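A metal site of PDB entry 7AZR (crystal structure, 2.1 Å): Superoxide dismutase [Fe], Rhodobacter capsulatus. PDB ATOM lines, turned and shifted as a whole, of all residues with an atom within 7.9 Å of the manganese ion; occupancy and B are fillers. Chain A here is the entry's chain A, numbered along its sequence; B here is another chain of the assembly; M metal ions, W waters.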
ATOM      1  N   HIS A  27      23.838  30.819  -4.827  1.00  0.00           N
ATOM      2  CA  HIS A  27      23.352  29.560  -5.393  1.00  0.00           C
ATOM      3  C   HIS A  27      22.909  28.612  -4.291  1.00  0.00           C
ATOM      4  O   HIS A  27      21.812  28.036  -4.374  1.00  0.00           O
ATOM      5  CB  HIS A  27      24.423  28.908  -6.262  1.00  0.00           C
ATOM      6  CG  HIS A  27      23.884  27.873  -7.196  1.00  0.00           C
ATOM      7  ND1 HIS A  27      24.681  27.258  -8.141  1.00  0.00           N
ATOM      8  CD2 HIS A  27      22.642  27.349  -7.351  1.00  0.00           C
ATOM      9  CE1 HIS A  27      23.960  26.393  -8.828  1.00  0.00           C
ATOM     10  NE2 HIS A  27      22.720  26.426  -8.356  1.00  0.00           N
ATOM     11  N   HIS A  28      23.733  28.467  -3.254  1.00  0.00           N
ATOM     12  CA  HIS A  28      23.429  27.587  -2.131  1.00  0.00           C
ATOM     13  C   HIS A  28      22.507  28.261  -1.108  1.00  0.00           C
ATOM     14  O   HIS A  28      21.507  27.671  -0.721  1.00  0.00           O
ATOM     15  CB  HIS A  28      24.713  27.100  -1.436  1.00  0.00           C
ATOM     16  CG  HIS A  28      24.469  26.307  -0.189  1.00  0.00           C
ATOM     17  ND1 HIS A  28      24.398  26.902   1.053  1.00  0.00           N
ATOM     18  CD2 HIS A  28      24.285  24.985   0.000  1.00  0.00           C
ATOM     19  CE1 HIS A  28      24.160  25.965   1.970  1.00  0.00           C
ATOM     20  NE2 HIS A  28      24.117  24.799   1.356  1.00  0.00           N
ATOM     21  N   HIS A  31      19.177  30.176  -3.672  1.00  0.00           N
ATOM     22  CA  HIS A  31      18.448  29.331  -4.619  1.00  0.00           C
ATOM     23  C   HIS A  31      18.089  27.956  -4.032  1.00  0.00           C
ATOM     24  O   HIS A  31      16.944  27.551  -4.045  1.00  0.00           O
ATOM     25  CB  HIS A  31      19.187  29.170  -5.946  1.00  0.00           C
ATOM     26  CG  HIS A  31      19.245  30.411  -6.783  1.00  0.00           C
ATOM     27  ND1 HIS A  31      18.249  30.743  -7.674  1.00  0.00           N
ATOM     28  CD2 HIS A  31      20.196  31.372  -6.893  1.00  0.00           C
ATOM     29  CE1 HIS A  31      18.583  31.867  -8.282  1.00  0.00           C
ATOM     30  NE2 HIS A  31      19.759  32.262  -7.845  1.00  0.00           N
ATOM     31  N   HIS A  32      19.092  27.249  -3.509  1.00  0.00           N
ATOM     32  CA  HIS A  32      18.839  25.910  -2.979  1.00  0.00           C
ATOM     33  C   HIS A  32      17.894  26.021  -1.764  1.00  0.00           C
ATOM     34  O   HIS A  32      16.960  25.248  -1.646  1.00  0.00           O
ATOM     35  CB  HIS A  32      20.131  25.161  -2.650  1.00  0.00           C
ATOM     36  CG  HIS A  32      19.933  23.715  -2.326  1.00  0.00           C
ATOM     37  ND1 HIS A  32      20.997  22.860  -2.108  1.00  0.00           N
ATOM     38  CD2 HIS A  32      18.809  22.978  -2.153  1.00  0.00           C
ATOM     39  CE1 HIS A  32      20.533  21.649  -1.845  1.00  0.00           C
ATOM     40  NE2 HIS A  32      19.205  21.696  -1.873  1.00  0.00           N
ATOM     41  N   TYR A  35      14.314  26.146  -2.854  1.00  0.00           N
ATOM     42  CA  TYR A  35      13.768  24.833  -3.225  1.00  0.00           C
ATOM     43  C   TYR A  35      13.361  24.029  -1.994  1.00  0.00           C
ATOM     44  O   TYR A  35      12.315  23.362  -1.979  1.00  0.00           O
ATOM     45  CB  TYR A  35      14.739  24.045  -4.093  1.00  0.00           C
ATOM     46  CG  TYR A  35      15.115  24.722  -5.383  1.00  0.00           C
ATOM     47  CD1 TYR A  35      14.134  25.255  -6.254  1.00  0.00           C
ATOM     48  CD2 TYR A  35      16.459  24.847  -5.753  1.00  0.00           C
ATOM     49  CE1 TYR A  35      14.487  25.861  -7.457  1.00  0.00           C
ATOM     50  CE2 TYR A  35      16.816  25.466  -6.953  1.00  0.00           C
ATOM     51  CZ  TYR A  35      15.830  25.970  -7.794  1.00  0.00           C
ATOM     52  OH  TYR A  35      16.190  26.574  -8.969  1.00  0.00           O
ATOM     53  N   GLN A  77      14.752  19.781  -7.772  1.00  0.00           N
ATOM     54  CA  GLN A  77      15.833  20.749  -7.655  1.00  0.00           C
ATOM     55  C   GLN A  77      16.591  20.613  -6.320  1.00  0.00           C
ATOM     56  O   GLN A  77      17.817  20.755  -6.293  1.00  0.00           O
ATOM     57  CB  GLN A  77      15.331  22.191  -7.905  1.00  0.00           C
ATOM     58  CG  GLN A  77      15.069  22.470  -9.380  1.00  0.00           C
ATOM     59  CD  GLN A  77      16.350  22.670 -10.166  1.00  0.00           C
ATOM     60  OE1 GLN A  77      17.065  21.697 -10.498  1.00  0.00           O
ATOM     61  NE2 GLN A  77      16.678  23.938 -10.443  1.00  0.00           N
ATOM     62  N   ASN A  80      18.804  17.625  -6.886  1.00  0.00           N
ATOM     63  CA  ASN A  80      19.836  17.953  -7.855  1.00  0.00           C
ATOM     64  C   ASN A  80      20.968  18.761  -7.219  1.00  0.00           C
ATOM     65  O   ASN A  80      22.151  18.453  -7.432  1.00  0.00           O
ATOM     66  CB  ASN A  80      19.299  18.738  -9.086  1.00  0.00           C
ATOM     67  CG  ASN A  80      18.219  17.983  -9.851  1.00  0.00           C
ATOM     68  OD1 ASN A  80      18.135  16.758  -9.742  1.00  0.00           O
ATOM     69  ND2 ASN A  80      17.364  18.708 -10.564  1.00  0.00           N
ATOM     70  N   HIS A  81      20.594  19.798  -6.469  1.00  0.00           N
ATOM     71  CA  HIS A  81      21.568  20.698  -5.847  1.00  0.00           C
ATOM     72  C   HIS A  81      22.370  19.963  -4.745  1.00  0.00           C
ATOM     73  O   HIS A  81      23.576  20.160  -4.627  1.00  0.00           O
ATOM     74  CB  HIS A  81      20.917  22.022  -5.369  1.00  0.00           C
ATOM     75  CG  HIS A  81      20.501  22.908  -6.492  1.00  0.00           C
ATOM     76  ND1 HIS A  81      19.353  22.686  -7.233  1.00  0.00           N
ATOM     77  CD2 HIS A  81      21.119  23.976  -7.079  1.00  0.00           C
ATOM     78  CE1 HIS A  81      19.264  23.575  -8.199  1.00  0.00           C
ATOM     79  NE2 HIS A  81      20.337  24.356  -8.158  1.00  0.00           N
ATOM     80  N   PHE A  84      24.941  18.030  -6.682  1.00  0.00           N
ATOM     81  CA  PHE A  84      25.849  18.992  -7.286  1.00  0.00           C
ATOM     82  C   PHE A  84      26.976  19.451  -6.325  1.00  0.00           C
ATOM     83  O   PHE A  84      28.154  19.379  -6.686  1.00  0.00           O
ATOM     84  CB  PHE A  84      25.024  20.194  -7.765  1.00  0.00           C
ATOM     85  CG  PHE A  84      25.771  21.170  -8.591  1.00  0.00           C
ATOM     86  CD1 PHE A  84      26.459  20.755  -9.737  1.00  0.00           C
ATOM     87  CD2 PHE A  84      25.743  22.520  -8.287  1.00  0.00           C
ATOM     88  CE1 PHE A  84      27.134  21.662 -10.523  1.00  0.00           C
ATOM     89  CE2 PHE A  84      26.418  23.427  -9.074  1.00  0.00           C
ATOM     90  CZ  PHE A  84      27.117  23.000 -10.189  1.00  0.00           C
ATOM     91  N   TRP A  85      26.610  19.895  -5.110  1.00  0.00           N
ATOM     92  CA  TRP A  85      27.631  20.359  -4.161  1.00  0.00           C
ATOM     93  C   TRP A  85      28.682  19.284  -3.841  1.00  0.00           C
ATOM     94  O   TRP A  85      29.865  19.592  -3.728  1.00  0.00           O
ATOM     95  CB  TRP A  85      27.049  20.895  -2.829  1.00  0.00           C
ATOM     96  CG  TRP A  85      25.896  21.812  -2.980  1.00  0.00           C
ATOM     97  CD1 TRP A  85      24.700  21.687  -2.347  1.00  0.00           C
ATOM     98  CD2 TRP A  85      25.810  22.981  -3.791  1.00  0.00           C
ATOM     99  NE1 TRP A  85      23.870  22.699  -2.703  1.00  0.00           N
ATOM    100  CE2 TRP A  85      24.511  23.523  -3.596  1.00  0.00           C
ATOM    101  CE3 TRP A  85      26.686  23.636  -4.673  1.00  0.00           C
ATOM    102  CZ2 TRP A  85      24.055  24.673  -4.276  1.00  0.00           C
ATOM    103  CZ3 TRP A  85      26.243  24.785  -5.332  1.00  0.00           C
ATOM    104  CH2 TRP A  85      24.930  25.290  -5.126  1.00  0.00           C
ATOM    105  N   GLY A 129      18.407  23.843 -17.135  1.00  0.00           N
ATOM    106  CA  GLY A 129      18.470  22.396 -16.911  1.00  0.00           C
ATOM    107  C   GLY A 129      19.828  21.926 -16.455  1.00  0.00           C
ATOM    108  O   GLY A 129      20.550  22.670 -15.818  1.00  0.00           O
ATOM    109  N   TRP A 130      20.148  20.680 -16.801  1.00  0.00           N
ATOM    110  CA  TRP A 130      21.273  19.923 -16.247  1.00  0.00           C
ATOM    111  C   TRP A 130      21.867  19.053 -17.326  1.00  0.00           C
ATOM    112  O   TRP A 130      21.111  18.530 -18.170  1.00  0.00           O
ATOM    113  CB  TRP A 130      20.782  19.018 -15.099  1.00  0.00           C
ATOM    114  CG  TRP A 130      20.322  19.779 -13.926  1.00  0.00           C
ATOM    115  CD1 TRP A 130      19.114  20.397 -13.782  1.00  0.00           C
ATOM    116  CD2 TRP A 130      21.080  20.091 -12.749  1.00  0.00           C
ATOM    117  NE1 TRP A 130      19.066  21.060 -12.589  1.00  0.00           N
ATOM    118  CE2 TRP A 130      20.259  20.904 -11.933  1.00  0.00           C
ATOM    119  CE3 TRP A 130      22.367  19.758 -12.292  1.00  0.00           C
ATOM    120  CZ2 TRP A 130      20.689  21.383 -10.684  1.00  0.00           C
ATOM    121  CZ3 TRP A 130      22.787  20.219 -11.052  1.00  0.00           C
ATOM    122  CH2 TRP A 130      21.963  21.025 -10.263  1.00  0.00           C
ATOM    123  N   ASN A 148      15.028  22.006 -16.578  1.00  0.00           N
ATOM    124  CA  ASN A 148      14.522  22.558 -15.339  1.00  0.00           C
ATOM    125  C   ASN A 148      15.031  21.707 -14.147  1.00  0.00           C
ATOM    126  O   ASN A 148      16.238  21.658 -13.922  1.00  0.00           O
ATOM    127  CB  ASN A 148      13.001  22.713 -15.440  1.00  0.00           C
ATOM    128  CG  ASN A 148      12.592  23.539 -16.650  1.00  0.00           C
ATOM    129  OD1 ASN A 148      13.283  24.508 -17.014  1.00  0.00           O
ATOM    130  ND2 ASN A 148      11.485  23.154 -17.295  1.00  0.00           N
ATOM    131  N   ASP A 164      24.839  21.805 -13.336  1.00  0.00           N
ATOM    132  CA  ASP A 164      23.739  22.764 -13.408  1.00  0.00           C
ATOM    133  C   ASP A 164      24.013  23.728 -14.542  1.00  0.00           C
ATOM    134  O   ASP A 164      25.063  24.386 -14.555  1.00  0.00           O
ATOM    135  CB  ASP A 164      23.702  23.502 -12.089  1.00  0.00           C
ATOM    136  CG  ASP A 164      22.458  24.329 -11.885  1.00  0.00           C
ATOM    137  OD1 ASP A 164      21.587  24.384 -12.770  1.00  0.00           O
ATOM    138  OD2 ASP A 164      22.388  24.908 -10.779  1.00  0.00           O
ATOM    139  N   VAL A 165      23.120  23.760 -15.542  1.00  0.00           N
ATOM    140  CA  VAL A 165      23.244  24.783 -16.602  1.00  0.00           C
ATOM    141  C   VAL A 165      22.119  25.818 -16.573  1.00  0.00           C
ATOM    142  O   VAL A 165      21.959  26.584 -17.493  1.00  0.00           O
ATOM    143  CB  VAL A 165      23.459  24.177 -18.002  1.00  0.00           C
ATOM    144  CG1 VAL A 165      24.789  23.435 -18.039  1.00  0.00           C
ATOM    145  CG2 VAL A 165      22.315  23.287 -18.411  1.00  0.00           C
ATOM    146  N   TRP A 166      21.366  25.883 -15.463  1.00  0.00           N
ATOM    147  CA  TRP A 166      20.615  27.087 -15.179  1.00  0.00           C
ATOM    148  C   TRP A 166      21.615  28.246 -15.146  1.00  0.00           C
ATOM    149  O   TRP A 166      22.736  28.094 -14.637  1.00  0.00           O
ATOM    150  CB  TRP A 166      19.913  27.033 -13.838  1.00  0.00           C
ATOM    151  CG  TRP A 166      18.715  26.159 -13.732  1.00  0.00           C
ATOM    152  CD1 TRP A 166      18.665  24.813 -13.955  1.00  0.00           C
ATOM    153  CD2 TRP A 166      17.413  26.547 -13.299  1.00  0.00           C
ATOM    154  NE1 TRP A 166      17.396  24.344 -13.681  1.00  0.00           N
ATOM    155  CE2 TRP A 166      16.611  25.389 -13.279  1.00  0.00           C
ATOM    156  CE3 TRP A 166      16.832  27.782 -12.917  1.00  0.00           C
ATOM    157  CZ2 TRP A 166      15.263  25.417 -12.919  1.00  0.00           C
ATOM    158  CZ3 TRP A 166      15.507  27.801 -12.542  1.00  0.00           C
ATOM    159  CH2 TRP A 166      14.738  26.632 -12.537  1.00  0.00           C
ATOM    160  N   GLU A 167      21.212  29.412 -15.652  1.00  0.00           N
ATOM    161  CA  GLU A 167      22.127  30.518 -15.795  1.00  0.00           C
ATOM    162  C   GLU A 167      22.667  31.022 -14.455  1.00  0.00           C
ATOM    163  O   GLU A 167      23.818  31.473 -14.396  1.00  0.00           O
ATOM    164  CB  GLU A 167      21.491  31.641 -16.640  1.00  0.00           C
ATOM    165  CG  GLU A 167      21.379  31.236 -18.124  1.00  0.00           C
ATOM    166  CD  GLU A 167      20.669  32.241 -18.996  1.00  0.00           C
ATOM    167  OE1 GLU A 167      19.662  32.790 -18.548  1.00  0.00           O
ATOM    168  OE2 GLU A 167      21.156  32.510 -20.121  1.00  0.00           O
ATOM    169  N   HIS A 168      21.873  30.904 -13.381  1.00  0.00           N
ATOM    170  CA  HIS A 168      22.322  31.342 -12.050  1.00  0.00           C
ATOM    171  C   HIS A 168      23.583  30.607 -11.583  1.00  0.00           C
ATOM    172  O   HIS A 168      24.336  31.128 -10.790  1.00  0.00           O
ATOM    173  CB  HIS A 168      21.228  31.312 -10.968  1.00  0.00           C
ATOM    174  CG  HIS A 168      20.687  29.944 -10.643  1.00  0.00           C
ATOM    175  ND1 HIS A 168      19.358  29.602 -10.813  1.00  0.00           N
ATOM    176  CD2 HIS A 168      21.301  28.830 -10.143  1.00  0.00           C
ATOM    177  CE1 HIS A 168      19.174  28.345 -10.421  1.00  0.00           C
ATOM    178  NE2 HIS A 168      20.342  27.854 -10.028  1.00  0.00           N
ATOM    179  N   SER A 169      23.806  29.392 -12.102  1.00  0.00           N
ATOM    180  CA  SER A 169      24.939  28.571 -11.709  1.00  0.00           C
ATOM    181  C   SER A 169      26.269  29.126 -12.188  1.00  0.00           C
ATOM    182  O   SER A 169      27.302  28.815 -11.599  1.00  0.00           O
ATOM    183  CB  SER A 169      24.774  27.138 -12.206  1.00  0.00           C
ATOM    184  OG  SER A 169      25.715  26.302 -11.569  1.00  0.00           O
ATOM    185  N   TYR A 170      26.251  29.950 -13.247  1.00  0.00           N
ATOM    186  CA  TYR A 170      27.453  30.439 -13.871  1.00  0.00           C
ATOM    187  C   TYR A 170      27.486  31.898 -14.248  1.00  0.00           C
ATOM    188  O   TYR A 170      28.550  32.407 -14.525  1.00  0.00           O
ATOM    189  CB  TYR A 170      27.806  29.611 -15.127  1.00  0.00           C
ATOM    190  CG  TYR A 170      26.782  29.621 -16.270  1.00  0.00           C
ATOM    191  CD1 TYR A 170      26.790  30.606 -17.256  1.00  0.00           C
ATOM    192  CD2 TYR A 170      25.819  28.621 -16.369  1.00  0.00           C
ATOM    193  CE1 TYR A 170      25.867  30.594 -18.294  1.00  0.00           C
ATOM    194  CE2 TYR A 170      24.896  28.609 -17.407  1.00  0.00           C
ATOM    195  CZ  TYR A 170      24.925  29.608 -18.377  1.00  0.00           C
ATOM    196  OH  TYR A 170      23.979  29.566 -19.398  1.00  0.00           O
ATOM    197  N   TYR A 181      32.265  27.670 -19.004  1.00  0.00           N
ATOM    198  CA  TYR A 181      31.878  27.210 -17.673  1.00  0.00           C
ATOM    199  C   TYR A 181      31.933  25.700 -17.571  1.00  0.00           C
ATOM    200  O   TYR A 181      32.496  25.158 -16.626  1.00  0.00           O
ATOM    201  CB  TYR A 181      30.500  27.736 -17.326  1.00  0.00           C
ATOM    202  CG  TYR A 181      29.730  26.987 -16.270  1.00  0.00           C
ATOM    203  CD1 TYR A 181      30.097  27.033 -14.919  1.00  0.00           C
ATOM    204  CD2 TYR A 181      28.592  26.271 -16.607  1.00  0.00           C
ATOM    205  CE1 TYR A 181      29.348  26.377 -13.947  1.00  0.00           C
ATOM    206  CE2 TYR A 181      27.841  25.609 -15.662  1.00  0.00           C
ATOM    207  CZ  TYR A 181      28.203  25.670 -14.337  1.00  0.00           C
ATOM    208  OH  TYR A 181      27.391  25.006 -13.422  1.00  0.00           O
ATOM    209  N   GLU B 167      17.051  33.989 -16.771  1.00  0.00           N
ATOM    210  CA  GLU B 167      17.861  34.611 -15.730  1.00  0.00           C
ATOM    211  C   GLU B 167      18.847  35.644 -16.273  1.00  0.00           C
ATOM    212  O   GLU B 167      19.119  36.650 -15.590  1.00  0.00           O
ATOM    213  CB  GLU B 167      18.541  33.530 -14.887  1.00  0.00           C
ATOM    214  CG  GLU B 167      17.576  32.829 -13.925  1.00  0.00           C
ATOM    215  CD  GLU B 167      18.202  31.682 -13.176  1.00  0.00           C
ATOM    216  OE1 GLU B 167      19.004  30.928 -13.778  1.00  0.00           O
ATOM    217  OE2 GLU B 167      17.908  31.544 -11.951  1.00  0.00           O
HETATM  218 MN    MN M   1      20.967  25.805  -9.577  1.00  0.00          MN
HETATM  219  O   HOH W   1      19.295  24.866 -10.997  1.00  0.00           O
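The manganese ion is bound by OD2 of Asp 164 (2.1 Å), NE2 of His 81 (2.1 Å), NE2 of His 168 (2.2 Å), NE2 of His 27 (2.2 Å) and water W1 (2.4 Å).
Water W1 lies within hydrogen-bond range of the side-chain amide nitrogen of Gln 77 (2.8 Å), the side-chain carboxylate of Asp 164 (2.9 Å) and the indole nitrogen of Trp 166 (3.3 Å).
The side-chain carboxylate (OD1) of Asp 164 sits at hydrogen-bond distance from the backbone NH (N) of Trp 166 (3.1 Å).
The backbone carbonyl oxygen of Asp 164 sits at hydrogen-bond distance from the side-chain hydroxyl of Tyr 181, at 2.7 Å.
A ring nitrogen (ND1) of His 81 lies within hydrogen-bond range of the backbone carbonyl oxygen of Gln 77 (2.6 Å).
The backbone carbonyl oxygen (O) of His 81 sits close to the indole nitrogen (NE1) of Trp 85, at 3.2 Å.
A ring nitrogen (ND1) of His 168 sits at hydrogen-bond distance from the side-chain carboxylate of Glu 167 of chain B, 2.7 Å away.
N of His 32 lies within hydrogen-bond range of O of His 27 (3.0 Å).
Within 4 Å of the manganese ion: His 27, His 81, Asp 164 and His 168.
The nearest printed residue that does not touch the manganese ion is Trp 166 (4.6 Å).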
